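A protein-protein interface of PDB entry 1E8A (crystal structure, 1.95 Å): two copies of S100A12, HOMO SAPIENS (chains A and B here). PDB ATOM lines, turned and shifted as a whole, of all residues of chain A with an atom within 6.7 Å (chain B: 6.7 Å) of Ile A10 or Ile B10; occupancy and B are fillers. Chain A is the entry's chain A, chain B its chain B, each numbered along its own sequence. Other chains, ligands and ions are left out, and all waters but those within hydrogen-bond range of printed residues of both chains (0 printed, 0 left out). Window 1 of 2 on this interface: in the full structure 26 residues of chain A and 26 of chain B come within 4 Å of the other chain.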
ATOM      1  N   LEU A   3     -28.521 -18.475 -12.239  1.00  0.00           N
ATOM      2  CA  LEU A   3     -28.346 -19.860 -11.844  1.00  0.00           C
ATOM      3  C   LEU A   3     -28.830 -20.846 -12.929  1.00  0.00           C
ATOM      4  O   LEU A   3     -28.200 -21.872 -13.242  1.00  0.00           O
ATOM      5  CB  LEU A   3     -29.139 -20.158 -10.567  1.00  0.00           C
ATOM      6  CG  LEU A   3     -28.576 -21.165  -9.587  1.00  0.00           C
ATOM      7  CD1 LEU A   3     -29.598 -21.901  -8.752  1.00  0.00           C
ATOM      8  CD2 LEU A   3     -27.409 -22.043 -10.037  1.00  0.00           C
ATOM      9  N   GLU A   5     -29.076 -20.326 -16.122  1.00  0.00           N
ATOM     10  CA  GLU A   5     -28.174 -20.325 -17.234  1.00  0.00           C
ATOM     11  C   GLU A   5     -26.987 -21.230 -16.919  1.00  0.00           C
ATOM     12  O   GLU A   5     -26.524 -21.916 -17.795  1.00  0.00           O
ATOM     13  CB  GLU A   5     -27.685 -18.927 -17.591  1.00  0.00           C
ATOM     14  CG  GLU A   5     -28.785 -17.982 -18.078  1.00  0.00           C
ATOM     15  CD  GLU A   5     -28.398 -16.503 -18.009  1.00  0.00           C
ATOM     16  OE1 GLU A   5     -27.245 -16.161 -17.660  1.00  0.00           O
ATOM     17  OE2 GLU A   5     -29.273 -15.653 -18.283  1.00  0.00           O
ATOM     18  N   HIS A   6     -26.452 -21.187 -15.698  1.00  0.00           N
ATOM     19  CA  HIS A   6     -25.326 -22.095 -15.398  1.00  0.00           C
ATOM     20  C   HIS A   6     -25.725 -23.554 -15.489  1.00  0.00           C
ATOM     21  O   HIS A   6     -24.986 -24.380 -16.052  1.00  0.00           O
ATOM     22  CB  HIS A   6     -24.686 -21.781 -14.026  1.00  0.00           C
ATOM     23  CG  HIS A   6     -23.910 -20.515 -14.028  1.00  0.00           C
ATOM     24  ND1 HIS A   6     -23.075 -20.184 -15.075  1.00  0.00           N
ATOM     25  CD2 HIS A   6     -23.988 -19.404 -13.242  1.00  0.00           C
ATOM     26  CE1 HIS A   6     -22.581 -18.970 -14.865  1.00  0.00           C
ATOM     27  NE2 HIS A   6     -23.053 -18.517 -13.714  1.00  0.00           N
ATOM     28  N   LEU A   7     -26.889 -23.886 -14.940  1.00  0.00           N
ATOM     29  CA  LEU A   7     -27.353 -25.231 -14.963  1.00  0.00           C
ATOM     30  C   LEU A   7     -27.500 -25.706 -16.413  1.00  0.00           C
ATOM     31  O   LEU A   7     -27.051 -26.809 -16.733  1.00  0.00           O
ATOM     32  CB  LEU A   7     -28.642 -25.405 -14.185  1.00  0.00           C
ATOM     33  CG  LEU A   7     -28.535 -25.131 -12.690  1.00  0.00           C
ATOM     34  CD1 LEU A   7     -29.926 -24.897 -12.086  1.00  0.00           C
ATOM     35  CD2 LEU A   7     -27.816 -26.254 -11.926  1.00  0.00           C
ATOM     36  N   GLU A   8     -28.095 -24.847 -17.261  1.00  0.00           N
ATOM     37  CA  GLU A   8     -28.306 -25.149 -18.646  1.00  0.00           C
ATOM     38  C   GLU A   8     -26.955 -25.300 -19.325  1.00  0.00           C
ATOM     39  O   GLU A   8     -26.810 -26.148 -20.196  1.00  0.00           O
ATOM     40  CB  GLU A   8     -29.075 -24.034 -19.316  1.00  0.00           C
ATOM     41  CG  GLU A   8     -29.067 -24.139 -20.839  1.00  0.00           C
ATOM     42  CD  GLU A   8     -29.725 -25.411 -21.405  1.00  0.00           C
ATOM     43  OE1 GLU A   8     -30.453 -26.122 -20.653  1.00  0.00           O
ATOM     44  OE2 GLU A   8     -29.480 -25.723 -22.636  1.00  0.00           O
ATOM     45  N   GLY A   9     -25.966 -24.528 -18.893  1.00  0.00           N
ATOM     46  CA  GLY A   9     -24.650 -24.603 -19.476  1.00  0.00           C
ATOM     47  C   GLY A   9     -23.985 -25.958 -19.226  1.00  0.00           C
ATOM     48  O   GLY A   9     -23.356 -26.536 -20.127  1.00  0.00           O
ATOM     49  N   ILE A  10     -24.137 -26.457 -18.022  1.00  0.00           N
ATOM     50  CA  ILE A  10     -23.659 -27.798 -17.630  1.00  0.00           C
ATOM     51  C   ILE A  10     -24.338 -28.886 -18.464  1.00  0.00           C
ATOM     52  O   ILE A  10     -23.677 -29.769 -18.989  1.00  0.00           O
ATOM     53  CB  ILE A  10     -23.842 -28.002 -16.147  1.00  0.00           C
ATOM     54  CG1 ILE A  10     -22.881 -27.068 -15.434  1.00  0.00           C
ATOM     55  CG2 ILE A  10     -23.563 -29.461 -15.726  1.00  0.00           C
ATOM     56  CD1 ILE A  10     -23.201 -26.877 -14.039  1.00  0.00           C
ATOM     57  N   VAL A  11     -25.661 -28.784 -18.628  1.00  0.00           N
ATOM     58  CA  VAL A  11     -26.356 -29.746 -19.449  1.00  0.00           C
ATOM     59  C   VAL A  11     -25.854 -29.658 -20.892  1.00  0.00           C
ATOM     60  O   VAL A  11     -25.633 -30.698 -21.537  1.00  0.00           O
ATOM     61  CB  VAL A  11     -27.875 -29.610 -19.398  1.00  0.00           C
ATOM     62  CG1 VAL A  11     -28.561 -30.624 -20.343  1.00  0.00           C
ATOM     63  CG2 VAL A  11     -28.399 -29.704 -17.981  1.00  0.00           C
ATOM     64  N   ASN A  12     -25.625 -28.440 -21.383  1.00  0.00           N
ATOM     65  CA  ASN A  12     -25.171 -28.259 -22.733  1.00  0.00           C
ATOM     66  C   ASN A  12     -23.820 -28.944 -22.903  1.00  0.00           C
ATOM     67  O   ASN A  12     -23.583 -29.599 -23.876  1.00  0.00           O
ATOM     68  CB  ASN A  12     -25.169 -26.754 -23.113  1.00  0.00           C
ATOM     69  CG  ASN A  12     -24.860 -26.472 -24.589  1.00  0.00           C
ATOM     70  OD1 ASN A  12     -25.231 -27.205 -25.501  1.00  0.00           O
ATOM     71  ND2 ASN A  12     -24.167 -25.334 -24.827  1.00  0.00           N
ATOM     72  N   ILE A  13     -22.943 -28.848 -21.929  1.00  0.00           N
ATOM     73  CA  ILE A  13     -21.600 -29.409 -22.035  1.00  0.00           C
ATOM     74  C   ILE A  13     -21.654 -30.924 -21.972  1.00  0.00           C
ATOM     75  O   ILE A  13     -20.934 -31.594 -22.666  1.00  0.00           O
ATOM     76  CB  ILE A  13     -20.639 -28.744 -21.033  1.00  0.00           C
ATOM     77  CG1 ILE A  13     -20.349 -27.279 -21.480  1.00  0.00           C
ATOM     78  CG2 ILE A  13     -19.333 -29.614 -20.911  1.00  0.00           C
ATOM     79  CD1 ILE A  13     -19.556 -26.397 -20.480  1.00  0.00           C
ATOM     80  N   PHE A  14     -22.566 -31.473 -21.198  1.00  0.00           N
ATOM     81  CA  PHE A  14     -22.788 -32.864 -21.187  1.00  0.00           C
ATOM     82  C   PHE A  14     -23.071 -33.333 -22.607  1.00  0.00           C
ATOM     83  O   PHE A  14     -22.470 -34.282 -23.089  1.00  0.00           O
ATOM     84  CB  PHE A  14     -23.937 -33.248 -20.243  1.00  0.00           C
ATOM     85  CG  PHE A  14     -24.362 -34.692 -20.359  1.00  0.00           C
ATOM     86  CD1 PHE A  14     -23.726 -35.685 -19.625  1.00  0.00           C
ATOM     87  CD2 PHE A  14     -25.412 -35.077 -21.202  1.00  0.00           C
ATOM     88  CE1 PHE A  14     -24.079 -36.993 -19.738  1.00  0.00           C
ATOM     89  CE2 PHE A  14     -25.794 -36.403 -21.284  1.00  0.00           C
ATOM     90  CZ  PHE A  14     -25.106 -37.388 -20.546  1.00  0.00           C
ATOM     91  N   HIS A  15     -23.995 -32.675 -23.279  1.00  0.00           N
ATOM     92  CA  HIS A  15     -24.304 -33.075 -24.632  1.00  0.00           C
ATOM     93  C   HIS A  15     -23.200 -32.740 -25.632  1.00  0.00           C
ATOM     94  O   HIS A  15     -23.040 -33.442 -26.644  1.00  0.00           O
ATOM     95  CB  HIS A  15     -25.629 -32.478 -25.087  1.00  0.00           C
ATOM     96  CG  HIS A  15     -26.815 -33.122 -24.454  1.00  0.00           C
ATOM     97  ND1 HIS A  15     -27.489 -32.521 -23.419  1.00  0.00           N
ATOM     98  CD2 HIS A  15     -27.202 -34.414 -24.430  1.00  0.00           C
ATOM     99  CE1 HIS A  15     -28.441 -33.344 -22.994  1.00  0.00           C
ATOM    100  NE2 HIS A  15     -28.350 -34.462 -23.679  1.00  0.00           N
ATOM    101  N   PHE A  70     -26.959 -39.321 -17.717  1.00  0.00           N
ATOM    102  CA  PHE A  70     -27.022 -37.977 -17.203  1.00  0.00           C
ATOM    103  C   PHE A  70     -27.074 -38.026 -15.684  1.00  0.00           C
ATOM    104  O   PHE A  70     -26.407 -37.281 -15.012  1.00  0.00           O
ATOM    105  CB  PHE A  70     -28.162 -37.087 -17.811  1.00  0.00           C
ATOM    106  CG  PHE A  70     -28.083 -35.674 -17.348  1.00  0.00           C
ATOM    107  CD1 PHE A  70     -27.064 -34.824 -17.837  1.00  0.00           C
ATOM    108  CD2 PHE A  70     -28.844 -35.232 -16.303  1.00  0.00           C
ATOM    109  CE1 PHE A  70     -26.902 -33.559 -17.342  1.00  0.00           C
ATOM    110  CE2 PHE A  70     -28.701 -33.902 -15.835  1.00  0.00           C
ATOM    111  CZ  PHE A  70     -27.741 -33.096 -16.330  1.00  0.00           C
ATOM    112  N   PHE A  73     -23.781 -38.718 -14.382  1.00  0.00           N
ATOM    113  CA  PHE A  73     -22.938 -37.561 -14.603  1.00  0.00           C
ATOM    114  C   PHE A  73     -23.182 -36.497 -13.511  1.00  0.00           C
ATOM    115  O   PHE A  73     -22.282 -35.713 -13.171  1.00  0.00           O
ATOM    116  CB  PHE A  73     -23.215 -36.989 -16.007  1.00  0.00           C
ATOM    117  CG  PHE A  73     -22.556 -35.691 -16.295  1.00  0.00           C
ATOM    118  CD1 PHE A  73     -21.283 -35.643 -16.761  1.00  0.00           C
ATOM    119  CD2 PHE A  73     -23.248 -34.511 -16.146  1.00  0.00           C
ATOM    120  CE1 PHE A  73     -20.684 -34.467 -17.080  1.00  0.00           C
ATOM    121  CE2 PHE A  73     -22.620 -33.307 -16.481  1.00  0.00           C
ATOM    122  CZ  PHE A  73     -21.354 -33.304 -16.917  1.00  0.00           C
ATOM    123  N   VAL A  77     -20.518 -33.744 -11.397  1.00  0.00           N
ATOM    124  CA  VAL A  77     -20.751 -32.324 -11.165  1.00  0.00           C
ATOM    125  C   VAL A  77     -20.610 -32.046  -9.678  1.00  0.00           C
ATOM    126  O   VAL A  77     -20.090 -31.015  -9.300  1.00  0.00           O
ATOM    127  CB  VAL A  77     -22.151 -31.896 -11.692  1.00  0.00           C
ATOM    128  CG1 VAL A  77     -22.553 -30.530 -11.184  1.00  0.00           C
ATOM    129  CG2 VAL A  77     -22.170 -31.922 -13.240  1.00  0.00           C
ATOM    130  N   LEU A  81     -17.999 -29.517  -8.157  1.00  0.00           N
ATOM    131  CA  LEU A  81     -18.453 -28.375  -7.337  1.00  0.00           C
ATOM    132  C   LEU A  81     -17.786 -28.355  -6.007  1.00  0.00           C
ATOM    133  O   LEU A  81     -17.411 -27.312  -5.516  1.00  0.00           O
ATOM    134  CB  LEU A  81     -19.978 -28.381  -7.121  1.00  0.00           C
ATOM    135  CG  LEU A  81     -20.828 -27.924  -8.258  1.00  0.00           C
ATOM    136  CD1 LEU A  81     -22.328 -28.342  -8.038  1.00  0.00           C
ATOM    137  CD2 LEU A  81     -20.681 -26.433  -8.610  1.00  0.00           C
ATOM    138  N   LEU B   3     -16.898 -25.109 -18.648  1.00  0.00           N
ATOM    139  CA  LEU B   3     -17.489 -25.886 -17.568  1.00  0.00           C
ATOM    140  C   LEU B   3     -17.060 -25.316 -16.226  1.00  0.00           C
ATOM    141  O   LEU B   3     -17.875 -25.147 -15.261  1.00  0.00           O
ATOM    142  CB  LEU B   3     -16.995 -27.321 -17.582  1.00  0.00           C
ATOM    143  CG  LEU B   3     -17.945 -28.466 -17.247  1.00  0.00           C
ATOM    144  CD1 LEU B   3     -17.199 -29.792 -16.980  1.00  0.00           C
ATOM    145  CD2 LEU B   3     -19.018 -28.195 -16.248  1.00  0.00           C
ATOM    146  N   GLU B   5     -16.168 -22.339 -15.566  1.00  0.00           N
ATOM    147  CA  GLU B   5     -16.844 -21.059 -15.361  1.00  0.00           C
ATOM    148  C   GLU B   5     -18.259 -21.274 -14.822  1.00  0.00           C
ATOM    149  O   GLU B   5     -18.688 -20.502 -13.974  1.00  0.00           O
ATOM    150  CB  GLU B   5     -16.855 -20.202 -16.620  1.00  0.00           C
ATOM    151  CG  GLU B   5     -15.496 -19.710 -17.090  1.00  0.00           C
ATOM    152  CD  GLU B   5     -15.575 -19.121 -18.489  1.00  0.00           C
ATOM    153  OE1 GLU B   5     -16.700 -19.196 -19.099  1.00  0.00           O
ATOM    154  OE2 GLU B   5     -14.523 -18.624 -19.004  1.00  0.00           O
ATOM    155  N   HIS B   6     -18.968 -22.333 -15.277  1.00  0.00           N
ATOM    156  CA  HIS B   6     -20.292 -22.632 -14.757  1.00  0.00           C
ATOM    157  C   HIS B   6     -20.233 -23.089 -13.340  1.00  0.00           C
ATOM    158  O   HIS B   6     -21.060 -22.664 -12.527  1.00  0.00           O
ATOM    159  CB  HIS B   6     -21.021 -23.658 -15.640  1.00  0.00           C
ATOM    160  CG  HIS B   6     -21.363 -23.116 -16.988  1.00  0.00           C
ATOM    161  ND1 HIS B   6     -22.039 -21.928 -17.157  1.00  0.00           N
ATOM    162  CD2 HIS B   6     -21.154 -23.613 -18.225  1.00  0.00           C
ATOM    163  CE1 HIS B   6     -22.238 -21.722 -18.444  1.00  0.00           C
ATOM    164  NE2 HIS B   6     -21.671 -22.718 -19.117  1.00  0.00           N
ATOM    165  N   LEU B   7     -19.267 -23.941 -13.016  1.00  0.00           N
ATOM    166  CA  LEU B   7     -19.052 -24.363 -11.645  1.00  0.00           C
ATOM    167  C   LEU B   7     -18.728 -23.200 -10.660  1.00  0.00           C
ATOM    168  O   LEU B   7     -19.341 -23.115  -9.582  1.00  0.00           O
ATOM    169  CB  LEU B   7     -17.967 -25.436 -11.587  1.00  0.00           C
ATOM    170  CG  LEU B   7     -18.204 -26.645 -12.478  1.00  0.00           C
ATOM    171  CD1 LEU B   7     -16.916 -27.424 -12.556  1.00  0.00           C
ATOM    172  CD2 LEU B   7     -19.278 -27.583 -11.930  1.00  0.00           C
ATOM    173  N   GLU B   8     -17.802 -22.326 -11.054  1.00  0.00           N
ATOM    174  CA  GLU B   8     -17.427 -21.188 -10.245  1.00  0.00           C
ATOM    175  C   GLU B   8     -18.656 -20.304 -10.048  1.00  0.00           C
ATOM    176  O   GLU B   8     -18.864 -19.695  -8.955  1.00  0.00           O
ATOM    177  CB  GLU B   8     -16.253 -20.405 -10.908  1.00  0.00           C
ATOM    178  CG  GLU B   8     -15.694 -19.259 -10.062  1.00  0.00           C
ATOM    179  CD  GLU B   8     -14.331 -18.740 -10.561  1.00  0.00           C
ATOM    180  OE1 GLU B   8     -13.748 -19.373 -11.451  1.00  0.00           O
ATOM    181  OE2 GLU B   8     -13.818 -17.709 -10.066  1.00  0.00           O
ATOM    182  N   GLY B   9     -19.457 -20.250 -11.105  1.00  0.00           N
ATOM    183  CA  GLY B   9     -20.665 -19.446 -11.152  1.00  0.00           C
ATOM    184  C   GLY B   9     -21.684 -19.964 -10.161  1.00  0.00           C
ATOM    185  O   GLY B   9     -22.337 -19.156  -9.431  1.00  0.00           O
ATOM    186  N   ILE B  10     -21.777 -21.276 -10.041  1.00  0.00           N
ATOM    187  CA  ILE B  10     -22.710 -21.855  -9.056  1.00  0.00           C
ATOM    188  C   ILE B  10     -22.239 -21.551  -7.613  1.00  0.00           C
ATOM    189  O   ILE B  10     -23.068 -21.238  -6.746  1.00  0.00           O
ATOM    190  CB  ILE B  10     -22.921 -23.323  -9.295  1.00  0.00           C
ATOM    191  CG1 ILE B  10     -23.623 -23.482 -10.636  1.00  0.00           C
ATOM    192  CG2 ILE B  10     -23.646 -23.975  -8.134  1.00  0.00           C
ATOM    193  CD1 ILE B  10     -23.824 -24.877 -11.069  1.00  0.00           C
ATOM    194  N   VAL B  11     -20.942 -21.694  -7.386  1.00  0.00           N
ATOM    195  CA  VAL B  11     -20.313 -21.340  -6.110  1.00  0.00           C
ATOM    196  C   VAL B  11     -20.592 -19.849  -5.756  1.00  0.00           C
ATOM    197  O   VAL B  11     -20.903 -19.495  -4.603  1.00  0.00           O
ATOM    198  CB  VAL B  11     -18.811 -21.585  -6.144  1.00  0.00           C
ATOM    199  CG1 VAL B  11     -18.123 -21.076  -4.867  1.00  0.00           C
ATOM    200  CG2 VAL B  11     -18.498 -23.061  -6.366  1.00  0.00           C
ATOM    201  N   ASN B  12     -20.402 -18.974  -6.739  1.00  0.00           N
ATOM    202  CA  ASN B  12     -20.633 -17.555  -6.559  1.00  0.00           C
ATOM    203  C   ASN B  12     -22.079 -17.296  -6.195  1.00  0.00           C
ATOM    204  O   ASN B  12     -22.354 -16.556  -5.283  1.00  0.00           O
ATOM    205  CB  ASN B  12     -20.231 -16.796  -7.819  1.00  0.00           C
ATOM    206  CG  ASN B  12     -18.732 -16.705  -7.961  1.00  0.00           C
ATOM    207  OD1 ASN B  12     -18.026 -16.816  -6.965  1.00  0.00           O
ATOM    208  ND2 ASN B  12     -18.224 -16.396  -9.172  1.00  0.00           N
ATOM    209  N   ILE B  13     -23.020 -17.956  -6.884  1.00  0.00           N
ATOM    210  CA  ILE B  13     -24.419 -17.721  -6.599  1.00  0.00           C
ATOM    211  C   ILE B  13     -24.799 -18.233  -5.216  1.00  0.00           C
ATOM    212  O   ILE B  13     -25.585 -17.604  -4.522  1.00  0.00           O
ATOM    213  CB  ILE B  13     -25.307 -18.260  -7.742  1.00  0.00           C
ATOM    214  CG1 ILE B  13     -25.137 -17.363  -8.966  1.00  0.00           C
ATOM    215  CG2 ILE B  13     -26.774 -18.347  -7.323  1.00  0.00           C
ATOM    216  CD1 ILE B  13     -25.671 -17.972 -10.290  1.00  0.00           C
ATOM    217  N   PHE B  14     -24.230 -19.358  -4.787  1.00  0.00           N
ATOM    218  CA  PHE B  14     -24.443 -19.822  -3.435  1.00  0.00           C
ATOM    219  C   PHE B  14     -24.022 -18.722  -2.437  1.00  0.00           C
ATOM    220  O   PHE B  14     -24.787 -18.351  -1.568  1.00  0.00           O
ATOM    221  CB  PHE B  14     -23.703 -21.138  -3.233  1.00  0.00           C
ATOM    222  CG  PHE B  14     -23.684 -21.628  -1.833  1.00  0.00           C
ATOM    223  CD1 PHE B  14     -24.680 -22.453  -1.358  1.00  0.00           C
ATOM    224  CD2 PHE B  14     -22.676 -21.294  -1.006  1.00  0.00           C
ATOM    225  CE1 PHE B  14     -24.662 -22.887  -0.053  1.00  0.00           C
ATOM    226  CE2 PHE B  14     -22.623 -21.757   0.278  1.00  0.00           C
ATOM    227  CZ  PHE B  14     -23.608 -22.570   0.761  1.00  0.00           C
ATOM    228  N   HIS B  15     -22.854 -18.129  -2.650  1.00  0.00           N
ATOM    229  CA  HIS B  15     -22.298 -17.102  -1.768  1.00  0.00           C
ATOM    230  C   HIS B  15     -23.098 -15.798  -1.860  1.00  0.00           C
ATOM    231  O   HIS B  15     -23.256 -15.124  -0.861  1.00  0.00           O
ATOM    232  CB  HIS B  15     -20.807 -16.834  -2.043  1.00  0.00           C
ATOM    233  CG  HIS B  15     -19.893 -17.892  -1.514  1.00  0.00           C
ATOM    234  ND1 HIS B  15     -18.793 -18.328  -2.214  1.00  0.00           N
ATOM    235  CD2 HIS B  15     -19.991 -18.695  -0.437  1.00  0.00           C
ATOM    236  CE1 HIS B  15     -18.141 -19.211  -1.476  1.00  0.00           C
ATOM    237  NE2 HIS B  15     -18.857 -19.459  -0.398  1.00  0.00           N
ATOM    238  N   LEU B  35     -32.796 -17.559  -2.416  1.00  0.00           N
ATOM    239  CA  LEU B  35     -32.113 -18.206  -3.526  1.00  0.00           C
ATOM    240  C   LEU B  35     -33.122 -18.952  -4.422  1.00  0.00           C
ATOM    241  O   LEU B  35     -33.145 -18.805  -5.665  1.00  0.00           O
ATOM    242  CB  LEU B  35     -31.050 -19.139  -2.984  1.00  0.00           C
ATOM    243  CG  LEU B  35     -30.154 -19.810  -4.056  1.00  0.00           C
ATOM    244  CD1 LEU B  35     -28.686 -20.085  -3.644  1.00  0.00           C
ATOM    245  CD2 LEU B  35     -30.796 -21.067  -4.570  1.00  0.00           C
ATOM    246  N   PHE B  70     -22.696 -26.056   1.908  1.00  0.00           N
ATOM    247  CA  PHE B  70     -22.505 -26.161   0.483  1.00  0.00           C
ATOM    248  C   PHE B  70     -22.680 -27.605   0.016  1.00  0.00           C
ATOM    249  O   PHE B  70     -23.192 -27.834  -1.053  1.00  0.00           O
ATOM    250  CB  PHE B  70     -21.178 -25.591   0.000  1.00  0.00           C
ATOM    251  CG  PHE B  70     -21.046 -25.614  -1.485  1.00  0.00           C
ATOM    252  CD1 PHE B  70     -21.663 -24.633  -2.247  1.00  0.00           C
ATOM    253  CD2 PHE B  70     -20.319 -26.588  -2.130  1.00  0.00           C
ATOM    254  CE1 PHE B  70     -21.560 -24.644  -3.618  1.00  0.00           C
ATOM    255  CE2 PHE B  70     -20.236 -26.588  -3.536  1.00  0.00           C
ATOM    256  CZ  PHE B  70     -20.849 -25.600  -4.255  1.00  0.00           C
ATOM    257  N   PHE B  73     -26.271 -28.144  -0.326  1.00  0.00           N
ATOM    258  CA  PHE B  73     -26.744 -27.385  -1.466  1.00  0.00           C
ATOM    259  C   PHE B  73     -26.516 -28.115  -2.771  1.00  0.00           C
ATOM    260  O   PHE B  73     -27.298 -27.972  -3.674  1.00  0.00           O
ATOM    261  CB  PHE B  73     -26.042 -26.031  -1.499  1.00  0.00           C
ATOM    262  CG  PHE B  73     -26.331 -25.186  -2.718  1.00  0.00           C
ATOM    263  CD1 PHE B  73     -27.528 -24.496  -2.848  1.00  0.00           C
ATOM    264  CD2 PHE B  73     -25.401 -25.031  -3.703  1.00  0.00           C
ATOM    265  CE1 PHE B  73     -27.763 -23.723  -3.930  1.00  0.00           C
ATOM    266  CE2 PHE B  73     -25.675 -24.226  -4.792  1.00  0.00           C
ATOM    267  CZ  PHE B  73     -26.826 -23.567  -4.866  1.00  0.00           C
ATOM    268  N   VAL B  77     -28.667 -28.513  -6.380  1.00  0.00           N
ATOM    269  CA  VAL B  77     -28.140 -28.461  -7.748  1.00  0.00           C
ATOM    270  C   VAL B  77     -28.463 -29.722  -8.518  1.00  0.00           C
ATOM    271  O   VAL B  77     -28.828 -29.627  -9.693  1.00  0.00           O
ATOM    272  CB  VAL B  77     -26.627 -28.175  -7.820  1.00  0.00           C
ATOM    273  CG1 VAL B  77     -26.126 -28.252  -9.243  1.00  0.00           C
ATOM    274  CG2 VAL B  77     -26.297 -26.845  -7.270  1.00  0.00           C
ATOM    275  N   LEU B  81     -30.541 -29.750 -11.936  1.00  0.00           N
ATOM    276  CA  LEU B  81     -29.918 -30.272 -13.150  1.00  0.00           C
ATOM    277  C   LEU B  81     -30.823 -31.252 -13.861  1.00  0.00           C
ATOM    278  O   LEU B  81     -30.896 -31.264 -15.095  1.00  0.00           O
ATOM    279  CB  LEU B  81     -28.582 -30.934 -12.835  1.00  0.00           C
ATOM    280  CG  LEU B  81     -27.426 -29.987 -12.668  1.00  0.00           C
ATOM    281  CD1 LEU B  81     -26.155 -30.713 -12.145  1.00  0.00           C
ATOM    282  CD2 LEU B  81     -27.154 -29.308 -14.015  1.00  0.00           C
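Of the printed residues of chain B, Ile A10 touches His B6 (3.9 Å), Ile B10 (3.6 Å) and Leu B81 (3.98 Å). Ile B10 touches just these residues of chain A: His A6 (3.9 Å), Ile A10 (3.6 Å) and Leu A81 (3.9 Å). Of the printed residues of chain A, Val B77 touches Leu A7 (3.7 Å) and Leu A81 (3.99 Å). Of the printed residues of chain A, Leu B81 touches Leu A7 (3.7 Å), Ile A10 (3.98 Å), Phe A70 (3.5 Å) and Val A77 (3.7 Å). Glu A8 touches none of the printed residues of chain B. The nearest printed residue of chain B that does not touch Ile A10 is Leu B3 (4.1 Å).
Leu A3 touches Ile B13, and with the chains exchanged Ile A13 touches Leu B3. His B6 touches its own counterpart, His A6. His A6 touches Ile B10, and with the chains exchanged Ile A10 touches His B6. Ile A10 touches Leu B81, and with the chains exchanged Leu A81 touches Ile B10. Positions printed for both chains: 3, 5, 6, 7, 8, 9, 10, 11, 12, 13, 14, 15, 70, 73, 77 and 81.
Among the printed residues, merely in contact across the chains: Ile A13 with Leu B3, Leu A3 with Ile B13, Phe A70 with Leu B81, Leu A81 with Phe B70, Gly A9 with His B6, His A6 with Gly B9, Ile A10 with Ile B10, His A6 with Ile B13, Leu A7 with Leu B81, Leu A81 with Leu B7, Val A77 with Leu B81, Leu A7 with Val B77, Leu A81 with Ile B10, Ile A10 with His B6, Ile A13 with His B6, His A6 with Ile B10, Ile A10 with Leu B81 and Leu A81 with Val B77.
Hydrophobic or aromatic side chains of chain A within 4 Å of the printed part of chain B: His A6, Leu A7, Ile A10, Ile A13, Phe A70, Val A77 and Leu A81. Of the 17 printed residues of chain B, 9 touch a printed residue of chain A. Printed residues of chain B that touch a printed residue of chain A: Leu B3, His B6, Leu B7, Gly B9, Ile B10, Ile B13, Phe B70, Val B77 and Leu B81. Hydrophobic or aromatic side chains of chain B within 4 Å of the printed part of chain A: Leu B3, His B6, Leu B7, Ile B10, Ile B13, Phe B70, Val B77 and Leu B81. Among the printed residues, 19 pairs touch across the chains. Among the printed residues, no Asp or Glu carboxylate lies within 4 Å of a Lys or Arg side-chain nitrogen of the other chain.
A ring nitrogen (ND1) of His A6 sits at hydrogen-bond distance from a ring nitrogen (ND1) of His B6, at 2.9 Å.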
